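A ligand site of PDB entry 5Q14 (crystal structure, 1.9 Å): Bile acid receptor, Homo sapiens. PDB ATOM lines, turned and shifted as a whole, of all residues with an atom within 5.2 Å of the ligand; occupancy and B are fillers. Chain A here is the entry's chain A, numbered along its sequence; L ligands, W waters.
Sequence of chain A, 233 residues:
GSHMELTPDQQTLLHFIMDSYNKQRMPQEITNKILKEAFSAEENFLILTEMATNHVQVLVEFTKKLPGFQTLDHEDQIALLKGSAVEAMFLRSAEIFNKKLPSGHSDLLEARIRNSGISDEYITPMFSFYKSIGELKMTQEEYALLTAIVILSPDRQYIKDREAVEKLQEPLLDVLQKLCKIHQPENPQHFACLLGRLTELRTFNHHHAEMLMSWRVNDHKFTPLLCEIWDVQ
Water W2 lies within hydrogen-bond range of an oxygen (O2) of the ligand, the backbone carbonyl oxygen of Met 51, the side-chain amide oxygen of Asn 54 and the guanidinium group of Arg 25.
Water W1 lies within hydrogen-bond range of O2 of the ligand and OE1 of Gln 24.
The side-chain hydroxyl of Tyr 130 lies close to the side-chain sulfur of Met 126, 3.6 Å away.
The side-chain hydroxyl of Ser 93 is in hydrogen-bond range of the backbone carbonyl oxygen of Met 89 (3.0 Å).
NH1 of Arg 92 lies close to NE2 of Gln 24 (3.3 Å).
O of Arg 25 sits at hydrogen-bond distance from NH2 of Arg 92, 2.8 Å away.
The backbone carbonyl oxygen (O) of Ile 34 lies within hydrogen-bond range of the guanidinium group (NH2) of Arg 112 (2.8 Å).
The backbone carbonyl oxygen of Ile 113 is in hydrogen-bond range of the side-chain hydroxyl of Ser 116 (2.7 Å).
The backbone carbonyl oxygen (O) of Ser 116 sits close to the side-chain amide nitrogen (ND2) of Asn 44 (3.4 Å).
The indole nitrogen (NE1) of Trp 215 sits at hydrogen-bond distance from the backbone carbonyl oxygen (O) of Ser 116 (3.2 Å).
The side-chain hydroxyl (OG) of Ser 93 sits close to a fluorine (F1) of the ligand.
N of Phe 97 lies close to F2 of the ligand (3.2 Å).
Ile 30 touches the ligand (CG2 to F3, 3.4 Å).
Thr 31 touches the ligand (CG2 to F3, 3.8 Å).
Ile 34 touches the ligand (CD1 to F3, 3.5 Å).
Asn 44 touches the ligand.
Ile 47 touches the ligand.
Leu 48 touches the ligand (CD1 to C28, 3.7 Å).
Met 51 touches the ligand.
CB of His 55 touches O2 of the ligand, 3.4 Å away.
CE of Met 89 touches C28 of the ligand, at 3.6 Å.
CE1 of Phe 90 touches C28 of the ligand (3.6 Å).
Ile 96 touches the ligand (CD1 to C15, 3.2 Å).
CD2 of Leu 109 touches F2 of the ligand (3.8 Å).
Ile 113 touches the ligand (CD1 to C22, 3.6 Å).
CB of Ser 116 touches C18 of the ligand, at 3.7 Å.
Ile 118 touches the ligand (CD1 to C26, 3.98 Å).
Met 126 touches the ligand (SD to C25, 3.6 Å).
CE of Met 211 touches CL1 of the ligand, 3.8 Å away.
Hydrophobic or aromatic side chains within 4 Å of the ligand: Ile 30, Ile 34, Ile 47, Leu 48, Met 51, His 55, Met 89, Phe 90, Ile 96, Phe 97, Leu 109, Ile 113, Ile 118, Met 126, Tyr 130 and Met 211.
21 residues have an atom within 4 Å of the ligand: Ile 30, Thr 31, Ile 34, Asn 44, Ile 47, Leu 48, Met 51, His 55, Met 89, Phe 90, Arg 92, Ser 93, Ile 96, Phe 97, Leu 109, Ile 113, Ser 116, Ile 118, Met 126, Tyr 130 and Met 211.
Along chain A the residues within 4 Å of the ligand span positions 30 to 211.
The side-chain hydroxyl of Tyr 130 is in hydrogen-bond range of a nitrogen (N2) of the ligand, 2.8 Å away.
An oxygen (O3) of the ligand is in salt-bridge range of the guanidinium group (NE) of Arg 92, at 3.3 Å.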
ATOM      1  N   GLN A  24     -11.974  -3.116   2.334  1.00  0.00           N
ATOM      2  CA  GLN A  24     -12.830  -4.141   2.920  1.00  0.00           C
ATOM      3  C   GLN A  24     -14.303  -3.947   2.598  1.00  0.00           C
ATOM      4  O   GLN A  24     -14.723  -2.866   2.158  1.00  0.00           O
ATOM      5  CB  GLN A  24     -12.679  -4.117   4.437  1.00  0.00           C
ATOM      6  CG  GLN A  24     -11.353  -4.596   4.940  1.00  0.00           C
ATOM      7  CD  GLN A  24     -11.320  -4.562   6.444  1.00  0.00           C
ATOM      8  OE1 GLN A  24     -11.311  -5.587   7.090  1.00  0.00           O
ATOM      9  NE2 GLN A  24     -11.344  -3.385   7.032  1.00  0.00           N
ATOM     10  N   ARG A  25     -15.125  -4.987   2.888  1.00  0.00           N
ATOM     11  CA  ARG A  25     -16.575  -4.907   2.713  1.00  0.00           C
ATOM     12  C   ARG A  25     -17.093  -3.898   3.723  1.00  0.00           C
ATOM     13  O   ARG A  25     -16.647  -3.897   4.874  1.00  0.00           O
ATOM     14  CB  ARG A  25     -17.219  -6.276   2.947  1.00  0.00           C
ATOM     15  CG  ARG A  25     -17.324  -7.125   1.710  1.00  0.00           C
ATOM     16  CD  ARG A  25     -18.054  -8.423   1.984  1.00  0.00           C
ATOM     17  NE  ARG A  25     -17.928  -9.352   0.854  1.00  0.00           N
ATOM     18  CZ  ARG A  25     -18.157 -10.655   0.939  1.00  0.00           C
ATOM     19  NH1 ARG A  25     -18.528 -11.199   2.090  1.00  0.00           N
ATOM     20  NH2 ARG A  25     -18.032 -11.421  -0.135  1.00  0.00           N
ATOM     21  N   ILE A  30     -22.681  -6.148   5.438  1.00  0.00           N
ATOM     22  CA  ILE A  30     -22.749  -7.307   6.332  1.00  0.00           C
ATOM     23  C   ILE A  30     -23.995  -7.268   7.233  1.00  0.00           C
ATOM     24  O   ILE A  30     -24.722  -8.255   7.283  1.00  0.00           O
ATOM     25  CB  ILE A  30     -21.413  -7.444   7.128  1.00  0.00           C
ATOM     26  CG1 ILE A  30     -20.252  -7.786   6.175  1.00  0.00           C
ATOM     27  CG2 ILE A  30     -21.504  -8.457   8.281  1.00  0.00           C
ATOM     28  CD1 ILE A  30     -19.166  -6.838   6.228  1.00  0.00           C
ATOM     29  N   THR A  31     -24.242  -6.138   7.926  1.00  0.00           N
ATOM     30  CA  THR A  31     -25.363  -6.004   8.855  1.00  0.00           C
ATOM     31  C   THR A  31     -26.711  -5.968   8.146  1.00  0.00           C
ATOM     32  O   THR A  31     -27.675  -6.496   8.696  1.00  0.00           O
ATOM     33  CB  THR A  31     -25.191  -4.825   9.819  1.00  0.00           C
ATOM     34  OG1 THR A  31     -25.039  -3.613   9.070  1.00  0.00           O
ATOM     35  CG2 THR A  31     -24.030  -5.035  10.766  1.00  0.00           C
ATOM     36  N   ILE A  34     -27.719  -9.629   7.457  1.00  0.00           N
ATOM     37  CA  ILE A  34     -28.124 -10.319   8.682  1.00  0.00           C
ATOM     38  C   ILE A  34     -29.459  -9.783   9.214  1.00  0.00           C
ATOM     39  O   ILE A  34     -30.254 -10.557   9.730  1.00  0.00           O
ATOM     40  CB  ILE A  34     -26.968 -10.289   9.747  1.00  0.00           C
ATOM     41  CG1 ILE A  34     -25.687 -10.947   9.188  1.00  0.00           C
ATOM     42  CG2 ILE A  34     -27.380 -10.926  11.086  1.00  0.00           C
ATOM     43  CD1 ILE A  34     -24.401 -10.641   9.970  1.00  0.00           C
ATOM     44  N   ASN A  44     -26.670 -19.929   7.598  1.00  0.00           N
ATOM     45  CA  ASN A  44     -25.716 -19.055   8.300  1.00  0.00           C
ATOM     46  C   ASN A  44     -24.298 -19.614   8.296  1.00  0.00           C
ATOM     47  O   ASN A  44     -23.356 -18.818   8.241  1.00  0.00           O
ATOM     48  CB  ASN A  44     -26.175 -18.752   9.724  1.00  0.00           C
ATOM     49  CG  ASN A  44     -27.256 -17.692   9.798  1.00  0.00           C
ATOM     50  OD1 ASN A  44     -27.228 -16.688   9.071  1.00  0.00           O
ATOM     51  ND2 ASN A  44     -28.197 -17.873  10.706  1.00  0.00           N
ATOM     52  N   ILE A  47     -22.945 -18.740   4.912  1.00  0.00           N
ATOM     53  CA  ILE A  47     -22.724 -17.279   4.903  1.00  0.00           C
ATOM     54  C   ILE A  47     -21.392 -17.017   5.628  1.00  0.00           C
ATOM     55  O   ILE A  47     -20.551 -16.296   5.116  1.00  0.00           O
ATOM     56  CB  ILE A  47     -23.931 -16.505   5.551  1.00  0.00           C
ATOM     57  CG1 ILE A  47     -25.187 -16.550   4.654  1.00  0.00           C
ATOM     58  CG2 ILE A  47     -23.548 -15.039   5.861  1.00  0.00           C
ATOM     59  CD1 ILE A  47     -26.537 -16.372   5.379  1.00  0.00           C
ATOM     60  N   LEU A  48     -21.198 -17.658   6.804  1.00  0.00           N
ATOM     61  CA  LEU A  48     -19.974 -17.519   7.589  1.00  0.00           C
ATOM     62  C   LEU A  48     -18.735 -17.932   6.805  1.00  0.00           C
ATOM     63  O   LEU A  48     -17.767 -17.166   6.772  1.00  0.00           O
ATOM     64  CB  LEU A  48     -20.054 -18.317   8.900  1.00  0.00           C
ATOM     65  CG  LEU A  48     -18.769 -18.355   9.762  1.00  0.00           C
ATOM     66  CD1 LEU A  48     -18.405 -16.956  10.314  1.00  0.00           C
ATOM     67  CD2 LEU A  48     -18.913 -19.354  10.868  1.00  0.00           C
ATOM     68  N   MET A  51     -17.986 -15.351   3.982  1.00  0.00           N
ATOM     69  CA  MET A  51     -17.478 -14.112   4.573  1.00  0.00           C
ATOM     70  C   MET A  51     -16.069 -14.279   5.123  1.00  0.00           C
ATOM     71  O   MET A  51     -15.241 -13.395   4.909  1.00  0.00           O
ATOM     72  CB  MET A  51     -18.414 -13.588   5.663  1.00  0.00           C
ATOM     73  CG  MET A  51     -19.707 -13.021   5.111  1.00  0.00           C
ATOM     74  SD  MET A  51     -20.786 -12.464   6.441  1.00  0.00           S
ATOM     75  CE  MET A  51     -19.999 -11.053   6.873  1.00  0.00           C
ATOM     76  N   ALA A  52     -15.790 -15.414   5.801  1.00  0.00           N
ATOM     77  CA  ALA A  52     -14.480 -15.708   6.370  1.00  0.00           C
ATOM     78  C   ALA A  52     -13.428 -15.902   5.295  1.00  0.00           C
ATOM     79  O   ALA A  52     -12.296 -15.457   5.469  1.00  0.00           O
ATOM     80  CB  ALA A  52     -14.545 -16.916   7.277  1.00  0.00           C
ATOM     81  N   ASN A  54     -13.547 -14.563   2.225  1.00  0.00           N
ATOM     82  CA  ASN A  54     -13.302 -13.225   1.667  1.00  0.00           C
ATOM     83  C   ASN A  54     -12.441 -12.399   2.622  1.00  0.00           C
ATOM     84  O   ASN A  54     -11.533 -11.706   2.167  1.00  0.00           O
ATOM     85  CB  ASN A  54     -14.621 -12.478   1.378  1.00  0.00           C
ATOM     86  CG  ASN A  54     -14.405 -11.033   0.979  1.00  0.00           C
ATOM     87  OD1 ASN A  54     -14.600 -10.100   1.784  1.00  0.00           O
ATOM     88  ND2 ASN A  54     -13.899 -10.829  -0.203  1.00  0.00           N
ATOM     89  N   HIS A  55     -12.701 -12.495   3.936  1.00  0.00           N
ATOM     90  CA  HIS A  55     -11.905 -11.740   4.917  1.00  0.00           C
ATOM     91  C   HIS A  55     -10.393 -12.111   4.829  1.00  0.00           C
ATOM     92  O   HIS A  55      -9.561 -11.197   4.870  1.00  0.00           O
ATOM     93  CB  HIS A  55     -12.421 -11.930   6.349  1.00  0.00           C
ATOM     94  CG  HIS A  55     -11.573 -11.201   7.343  1.00  0.00           C
ATOM     95  ND1 HIS A  55     -10.478 -11.808   7.917  1.00  0.00           N
ATOM     96  CD2 HIS A  55     -11.646  -9.922   7.796  1.00  0.00           C
ATOM     97  CE1 HIS A  55      -9.916 -10.889   8.698  1.00  0.00           C
ATOM     98  NE2 HIS A  55     -10.604  -9.748   8.678  1.00  0.00           N
ATOM     99  N   MET A  89     -10.035 -11.269  12.056  1.00  0.00           N
ATOM    100  CA  MET A  89     -11.456 -11.432  11.741  1.00  0.00           C
ATOM    101  C   MET A  89     -12.359 -11.063  12.923  1.00  0.00           C
ATOM    102  O   MET A  89     -13.363 -10.365  12.713  1.00  0.00           O
ATOM    103  CB  MET A  89     -11.776 -12.822  11.213  1.00  0.00           C
ATOM    104  CG  MET A  89     -12.962 -12.741  10.258  1.00  0.00           C
ATOM    105  SD  MET A  89     -13.664 -14.320   9.821  1.00  0.00           S
ATOM    106  CE  MET A  89     -14.217 -14.837  11.367  1.00  0.00           C
ATOM    107  N   PHE A  90     -11.998 -11.496  14.137  1.00  0.00           N
ATOM    108  CA  PHE A  90     -12.786 -11.130  15.327  1.00  0.00           C
ATOM    109  C   PHE A  90     -12.704  -9.652  15.659  1.00  0.00           C
ATOM    110  O   PHE A  90     -13.664  -9.092  16.158  1.00  0.00           O
ATOM    111  CB  PHE A  90     -12.426 -12.003  16.536  1.00  0.00           C
ATOM    112  CG  PHE A  90     -13.074 -13.351  16.420  1.00  0.00           C
ATOM    113  CD1 PHE A  90     -14.465 -13.489  16.532  1.00  0.00           C
ATOM    114  CD2 PHE A  90     -12.319 -14.478  16.170  1.00  0.00           C
ATOM    115  CE1 PHE A  90     -15.057 -14.746  16.417  1.00  0.00           C
ATOM    116  CE2 PHE A  90     -12.919 -15.739  16.050  1.00  0.00           C
ATOM    117  CZ  PHE A  90     -14.276 -15.861  16.154  1.00  0.00           C
ATOM    118  N   ARG A  92     -12.399  -7.276  13.331  1.00  0.00           N
ATOM    119  CA  ARG A  92     -13.275  -6.682  12.321  1.00  0.00           C
ATOM    120  C   ARG A  92     -14.751  -6.934  12.681  1.00  0.00           C
ATOM    121  O   ARG A  92     -15.567  -6.037  12.500  1.00  0.00           O
ATOM    122  CB  ARG A  92     -12.979  -7.229  10.905  1.00  0.00           C
ATOM    123  CG  ARG A  92     -13.050  -6.193   9.770  1.00  0.00           C
ATOM    124  CD  ARG A  92     -14.253  -5.282   9.759  1.00  0.00           C
ATOM    125  NE  ARG A  92     -14.581  -4.764   8.427  1.00  0.00           N
ATOM    126  CZ  ARG A  92     -14.536  -3.490   8.062  1.00  0.00           C
ATOM    127  NH1 ARG A  92     -14.021  -2.580   8.876  1.00  0.00           N
ATOM    128  NH2 ARG A  92     -14.893  -3.130   6.855  1.00  0.00           N
ATOM    129  N   SER A  93     -15.078  -8.121  13.227  1.00  0.00           N
ATOM    130  CA  SER A  93     -16.450  -8.443  13.653  1.00  0.00           C
ATOM    131  C   SER A  93     -16.872  -7.504  14.795  1.00  0.00           C
ATOM    132  O   SER A  93     -18.009  -7.011  14.791  1.00  0.00           O
ATOM    133  CB  SER A  93     -16.522  -9.892  14.125  1.00  0.00           C
ATOM    134  OG  SER A  93     -16.314 -10.792  13.048  1.00  0.00           O
ATOM    135  N   ILE A  96     -17.631  -4.056  13.296  1.00  0.00           N
ATOM    136  CA  ILE A  96     -18.941  -4.135  12.635  1.00  0.00           C
ATOM    137  C   ILE A  96     -20.052  -4.139  13.686  1.00  0.00           C
ATOM    138  O   ILE A  96     -21.013  -3.386  13.536  1.00  0.00           O
ATOM    139  CB  ILE A  96     -19.037  -5.344  11.688  1.00  0.00           C
ATOM    140  CG1 ILE A  96     -18.082  -5.193  10.488  1.00  0.00           C
ATOM    141  CG2 ILE A  96     -20.480  -5.557  11.194  1.00  0.00           C
ATOM    142  CD1 ILE A  96     -17.872  -6.442   9.706  1.00  0.00           C
ATOM    143  N   PHE A  97     -19.917  -4.942  14.758  1.00  0.00           N
ATOM    144  CA  PHE A  97     -20.917  -5.024  15.822  1.00  0.00           C
ATOM    145  C   PHE A  97     -21.168  -3.680  16.533  1.00  0.00           C
ATOM    146  O   PHE A  97     -22.299  -3.409  16.927  1.00  0.00           O
ATOM    147  CB  PHE A  97     -20.598  -6.143  16.839  1.00  0.00           C
ATOM    148  CG  PHE A  97     -21.705  -6.359  17.847  1.00  0.00           C
ATOM    149  CD1 PHE A  97     -22.917  -6.904  17.459  1.00  0.00           C
ATOM    150  CD2 PHE A  97     -21.553  -5.939  19.165  1.00  0.00           C
ATOM    151  CE1 PHE A  97     -23.982  -6.993  18.368  1.00  0.00           C
ATOM    152  CE2 PHE A  97     -22.597  -6.095  20.089  1.00  0.00           C
ATOM    153  CZ  PHE A  97     -23.803  -6.610  19.687  1.00  0.00           C
ATOM    154  N   LEU A 109     -29.635  -7.563  15.520  1.00  0.00           N
ATOM    155  CA  LEU A 109     -28.357  -8.073  15.008  1.00  0.00           C
ATOM    156  C   LEU A 109     -27.743  -9.059  16.014  1.00  0.00           C
ATOM    157  O   LEU A 109     -27.349 -10.160  15.627  1.00  0.00           O
ATOM    158  CB  LEU A 109     -27.374  -6.914  14.726  1.00  0.00           C
ATOM    159  CG  LEU A 109     -26.005  -7.324  14.160  1.00  0.00           C
ATOM    160  CD1 LEU A 109     -26.126  -7.862  12.711  1.00  0.00           C
ATOM    161  CD2 LEU A 109     -25.048  -6.197  14.249  1.00  0.00           C
ATOM    162  N   ARG A 112     -29.942 -12.217  16.175  1.00  0.00           N
ATOM    163  CA  ARG A 112     -29.740 -13.020  14.953  1.00  0.00           C
ATOM    164  C   ARG A 112     -28.433 -13.827  15.001  1.00  0.00           C
ATOM    165  O   ARG A 112     -28.417 -14.997  14.643  1.00  0.00           O
ATOM    166  CB  ARG A 112     -29.817 -12.141  13.697  1.00  0.00           C
ATOM    167  CG  ARG A 112     -31.224 -11.623  13.349  1.00  0.00           C
ATOM    168  CD  ARG A 112     -31.929 -12.474  12.315  1.00  0.00           C
ATOM    169  NE  ARG A 112     -33.342 -12.121  12.145  1.00  0.00           N
ATOM    170  CZ  ARG A 112     -33.786 -11.165  11.328  1.00  0.00           C
ATOM    171  NH1 ARG A 112     -35.088 -10.932  11.205  1.00  0.00           N
ATOM    172  NH2 ARG A 112     -32.931 -10.433  10.632  1.00  0.00           N
ATOM    173  N   ILE A 113     -27.345 -13.220  15.489  1.00  0.00           N
ATOM    174  CA  ILE A 113     -26.024 -13.866  15.638  1.00  0.00           C
ATOM    175  C   ILE A 113     -26.091 -14.919  16.755  1.00  0.00           C
ATOM    176  O   ILE A 113     -25.534 -16.003  16.602  1.00  0.00           O
ATOM    177  CB  ILE A 113     -24.899 -12.821  15.869  1.00  0.00           C
ATOM    178  CG1 ILE A 113     -24.786 -11.847  14.655  1.00  0.00           C
ATOM    179  CG2 ILE A 113     -23.542 -13.516  16.156  1.00  0.00           C
ATOM    180  CD1 ILE A 113     -24.092 -10.532  14.947  1.00  0.00           C
ATOM    181  N   SER A 116     -27.679 -17.947  15.293  1.00  0.00           N
ATOM    182  CA  SER A 116     -27.139 -18.280  13.971  1.00  0.00           C
ATOM    183  C   SER A 116     -26.747 -19.754  13.788  1.00  0.00           C
ATOM    184  O   SER A 116     -26.578 -20.183  12.650  1.00  0.00           O
ATOM    185  CB  SER A 116     -25.968 -17.375  13.623  1.00  0.00           C
ATOM    186  OG  SER A 116     -24.905 -17.558  14.529  1.00  0.00           O
ATOM    187  N   ILE A 118     -24.238 -21.045  16.102  1.00  0.00           N
ATOM    188  CA  ILE A 118     -23.058 -21.047  16.977  1.00  0.00           C
ATOM    189  C   ILE A 118     -23.444 -21.637  18.367  1.00  0.00           C
ATOM    190  O   ILE A 118     -24.517 -21.315  18.890  1.00  0.00           O
ATOM    191  CB  ILE A 118     -22.442 -19.621  17.091  1.00  0.00           C
ATOM    192  CG1 ILE A 118     -21.158 -19.635  17.958  1.00  0.00           C
ATOM    193  CG2 ILE A 118     -23.463 -18.566  17.580  1.00  0.00           C
ATOM    194  CD1 ILE A 118     -20.318 -18.410  17.885  1.00  0.00           C
ATOM    195  N   MET A 126     -17.758 -14.338  23.065  1.00  0.00           N
ATOM    196  CA  MET A 126     -17.706 -13.554  21.823  1.00  0.00           C
ATOM    197  C   MET A 126     -18.333 -12.155  22.016  1.00  0.00           C
ATOM    198  O   MET A 126     -17.698 -11.155  21.707  1.00  0.00           O
ATOM    199  CB  MET A 126     -18.411 -14.329  20.700  1.00  0.00           C
ATOM    200  CG  MET A 126     -18.380 -13.616  19.368  1.00  0.00           C
ATOM    201  SD  MET A 126     -19.337 -14.440  18.071  1.00  0.00           S
ATOM    202  CE  MET A 126     -20.944 -14.264  18.692  1.00  0.00           C
ATOM    203  N   TYR A 130     -16.871  -8.278  22.082  1.00  0.00           N
ATOM    204  CA  TYR A 130     -17.408  -7.205  21.230  1.00  0.00           C
ATOM    205  C   TYR A 130     -17.845  -6.021  22.070  1.00  0.00           C
ATOM    206  O   TYR A 130     -17.590  -4.879  21.683  1.00  0.00           O
ATOM    207  CB  TYR A 130     -18.606  -7.691  20.376  1.00  0.00           C
ATOM    208  CG  TYR A 130     -18.323  -8.773  19.350  1.00  0.00           C
ATOM    209  CD1 TYR A 130     -17.025  -9.070  18.954  1.00  0.00           C
ATOM    210  CD2 TYR A 130     -19.370  -9.482  18.768  1.00  0.00           C
ATOM    211  CE1 TYR A 130     -16.774 -10.038  17.990  1.00  0.00           C
ATOM    212  CE2 TYR A 130     -19.129 -10.461  17.811  1.00  0.00           C
ATOM    213  CZ  TYR A 130     -17.827 -10.736  17.412  1.00  0.00           C
ATOM    214  OH  TYR A 130     -17.561 -11.722  16.508  1.00  0.00           O
ATOM    215  N   MET A 211     -15.339 -23.467  17.299  1.00  0.00           N
ATOM    216  CA  MET A 211     -16.482 -22.584  16.999  1.00  0.00           C
ATOM    217  C   MET A 211     -17.098 -22.949  15.655  1.00  0.00           C
ATOM    218  O   MET A 211     -18.323 -22.846  15.488  1.00  0.00           O
ATOM    219  CB  MET A 211     -16.086 -21.109  17.031  1.00  0.00           C
ATOM    220  CG  MET A 211     -15.964 -20.560  18.420  1.00  0.00           C
ATOM    221  SD  MET A 211     -15.268 -18.892  18.454  1.00  0.00           S
ATOM    222  CE  MET A 211     -16.699 -17.901  18.160  1.00  0.00           C
ATOM    223  N   LEU A 212     -16.252 -23.397  14.707  1.00  0.00           N
ATOM    224  CA  LEU A 212     -16.706 -23.820  13.400  1.00  0.00           C
ATOM    225  C   LEU A 212     -17.237 -25.226  13.462  1.00  0.00           C
ATOM    226  O   LEU A 212     -18.313 -25.459  12.941  1.00  0.00           O
ATOM    227  CB  LEU A 212     -15.581 -23.721  12.360  1.00  0.00           C
ATOM    228  CG  LEU A 212     -15.005 -22.337  12.034  1.00  0.00           C
ATOM    229  CD1 LEU A 212     -14.032 -22.434  10.889  1.00  0.00           C
ATOM    230  CD2 LEU A 212     -16.090 -21.337  11.658  1.00  0.00           C
ATOM    231  N   TRP A 215     -20.789 -25.768  15.164  1.00  0.00           N
ATOM    232  CA  TRP A 215     -21.928 -25.090  14.546  1.00  0.00           C
ATOM    233  C   TRP A 215     -23.054 -26.130  14.386  1.00  0.00           C
ATOM    234  O   TRP A 215     -22.791 -27.259  13.951  1.00  0.00           O
ATOM    235  CB  TRP A 215     -21.563 -24.492  13.190  1.00  0.00           C
ATOM    236  CG  TRP A 215     -22.438 -23.349  12.798  1.00  0.00           C
ATOM    237  CD1 TRP A 215     -23.658 -23.420  12.190  1.00  0.00           C
ATOM    238  CD2 TRP A 215     -22.185 -21.956  13.025  1.00  0.00           C
ATOM    239  NE1 TRP A 215     -24.164 -22.161  11.989  1.00  0.00           N
ATOM    240  CE2 TRP A 215     -23.275 -21.236  12.487  1.00  0.00           C
ATOM    241  CE3 TRP A 215     -21.117 -21.242  13.608  1.00  0.00           C
ATOM    242  CZ2 TRP A 215     -23.323 -19.842  12.501  1.00  0.00           C
ATOM    243  CZ3 TRP A 215     -21.197 -19.851  13.663  1.00  0.00           C
ATOM    244  CH2 TRP A 215     -22.294 -19.174  13.130  1.00  0.00           C
ATOM    245  N   TRP A 230      -7.954 -21.743   9.519  1.00  0.00           N
ATOM    246  CA  TRP A 230      -8.701 -22.053  10.749  1.00  0.00           C
ATOM    247  C   TRP A 230      -8.385 -23.386  11.400  1.00  0.00           C
ATOM    248  O   TRP A 230      -8.924 -23.671  12.475  1.00  0.00           O
ATOM    249  CB  TRP A 230     -10.220 -21.936  10.512  1.00  0.00           C
ATOM    250  CG  TRP A 230     -10.701 -20.527  10.374  1.00  0.00           C
ATOM    251  CD1 TRP A 230     -10.495 -19.687   9.329  1.00  0.00           C
ATOM    252  CD2 TRP A 230     -11.547 -19.826  11.298  1.00  0.00           C
ATOM    253  NE1 TRP A 230     -11.109 -18.478   9.561  1.00  0.00           N
ATOM    254  CE2 TRP A 230     -11.752 -18.530  10.769  1.00  0.00           C
ATOM    255  CE3 TRP A 230     -12.081 -20.124  12.569  1.00  0.00           C
ATOM    256  CZ2 TRP A 230     -12.531 -17.578  11.414  1.00  0.00           C
ATOM    257  CZ3 TRP A 230     -12.864 -19.177  13.201  1.00  0.00           C
ATOM    258  CH2 TRP A 230     -13.085 -17.911  12.633  1.00  0.00           C
HETATM  259  N1  LIG L   1     -20.155 -12.572  12.476  1.00  0.00           N
HETATM  260  N2  LIG L   1     -19.466 -11.926  14.520  1.00  0.00           N
HETATM  261  C1  LIG L   1     -20.612 -11.270  12.649  1.00  0.00           C
HETATM  262  C2  LIG L   1     -20.182 -10.881  13.913  1.00  0.00           C
HETATM  263  C3  LIG L   1     -21.359 -10.434  11.824  1.00  0.00           C
HETATM  264  C4  LIG L   1     -20.335 -13.489  11.280  1.00  0.00           C
HETATM  265  C5  LIG L   1     -20.493  -9.605  14.392  1.00  0.00           C
HETATM  266  C6  LIG L   1     -15.406  -8.967   7.226  1.00  0.00           C
HETATM  267  C7  LIG L   1     -16.135  -9.950   8.079  1.00  0.00           C
HETATM  268  C8  LIG L   1     -17.641 -10.394   9.875  1.00  0.00           C
HETATM  269  C9  LIG L   1     -17.532 -11.761   9.690  1.00  0.00           C
HETATM  270  C10 LIG L   1     -16.019 -11.327   7.864  1.00  0.00           C
HETATM  271  C11 LIG L   1     -16.706 -12.241   8.666  1.00  0.00           C
HETATM  272  C12 LIG L   1     -21.813 -13.816  11.029  1.00  0.00           C
HETATM  273  C13 LIG L   1     -17.580 -14.474  13.289  1.00  0.00           C
HETATM  274  C14 LIG L   1     -19.623 -12.872  10.076  1.00  0.00           C
HETATM  275  O1  LIG L   1     -18.273 -12.541  10.535  1.00  0.00           O
HETATM  276  C15 LIG L   1     -16.962  -9.484   9.093  1.00  0.00           C
HETATM  277  F1  LIG L   1     -18.437  -9.941  10.863  1.00  0.00           F
HETATM  278  O2  LIG L   1     -14.721  -9.469   6.266  1.00  0.00           O
HETATM  279  O3  LIG L   1     -15.480  -7.769   7.436  1.00  0.00           O
HETATM  280  C16 LIG L   1     -21.979 -14.872   9.922  1.00  0.00           C
HETATM  281  C17 LIG L   1     -23.452 -15.200   9.638  1.00  0.00           C
HETATM  282  C18 LIG L   1     -24.164 -15.678  10.892  1.00  0.00           C
HETATM  283  C19 LIG L   1     -24.013 -14.642  12.043  1.00  0.00           C
HETATM  284  C20 LIG L   1     -22.520 -14.298  12.299  1.00  0.00           C
HETATM  285  C21 LIG L   1     -21.650  -9.184  12.308  1.00  0.00           C
HETATM  286  C22 LIG L   1     -21.219  -8.778  13.557  1.00  0.00           C
HETATM  287  C23 LIG L   1     -19.481 -12.910  13.627  1.00  0.00           C
HETATM  288  C24 LIG L   1     -18.841 -14.211  13.834  1.00  0.00           C
HETATM  289  C25 LIG L   1     -19.469 -15.220  14.551  1.00  0.00           C
HETATM  290  C26 LIG L   1     -18.867 -16.463  14.734  1.00  0.00           C
HETATM  291  C27 LIG L   1     -17.611 -16.684  14.188  1.00  0.00           C
HETATM  292  C28 LIG L   1     -16.966 -15.706  13.465  1.00  0.00           C
HETATM  293 CL1  LIG L   1     -16.850 -18.226  14.405  1.00  0.00          CL
HETATM  294  F2  LIG L   1     -21.545  -7.539  13.977  1.00  0.00           F
HETATM  295  F3  LIG L   1     -22.361  -8.321  11.533  1.00  0.00           F
HETATM  296  O   HOH W   1     -13.062  -7.545   5.258  1.00  0.00           O
HETATM  297  O   HOH W   2     -15.990 -10.846   4.335  1.00  0.00           O
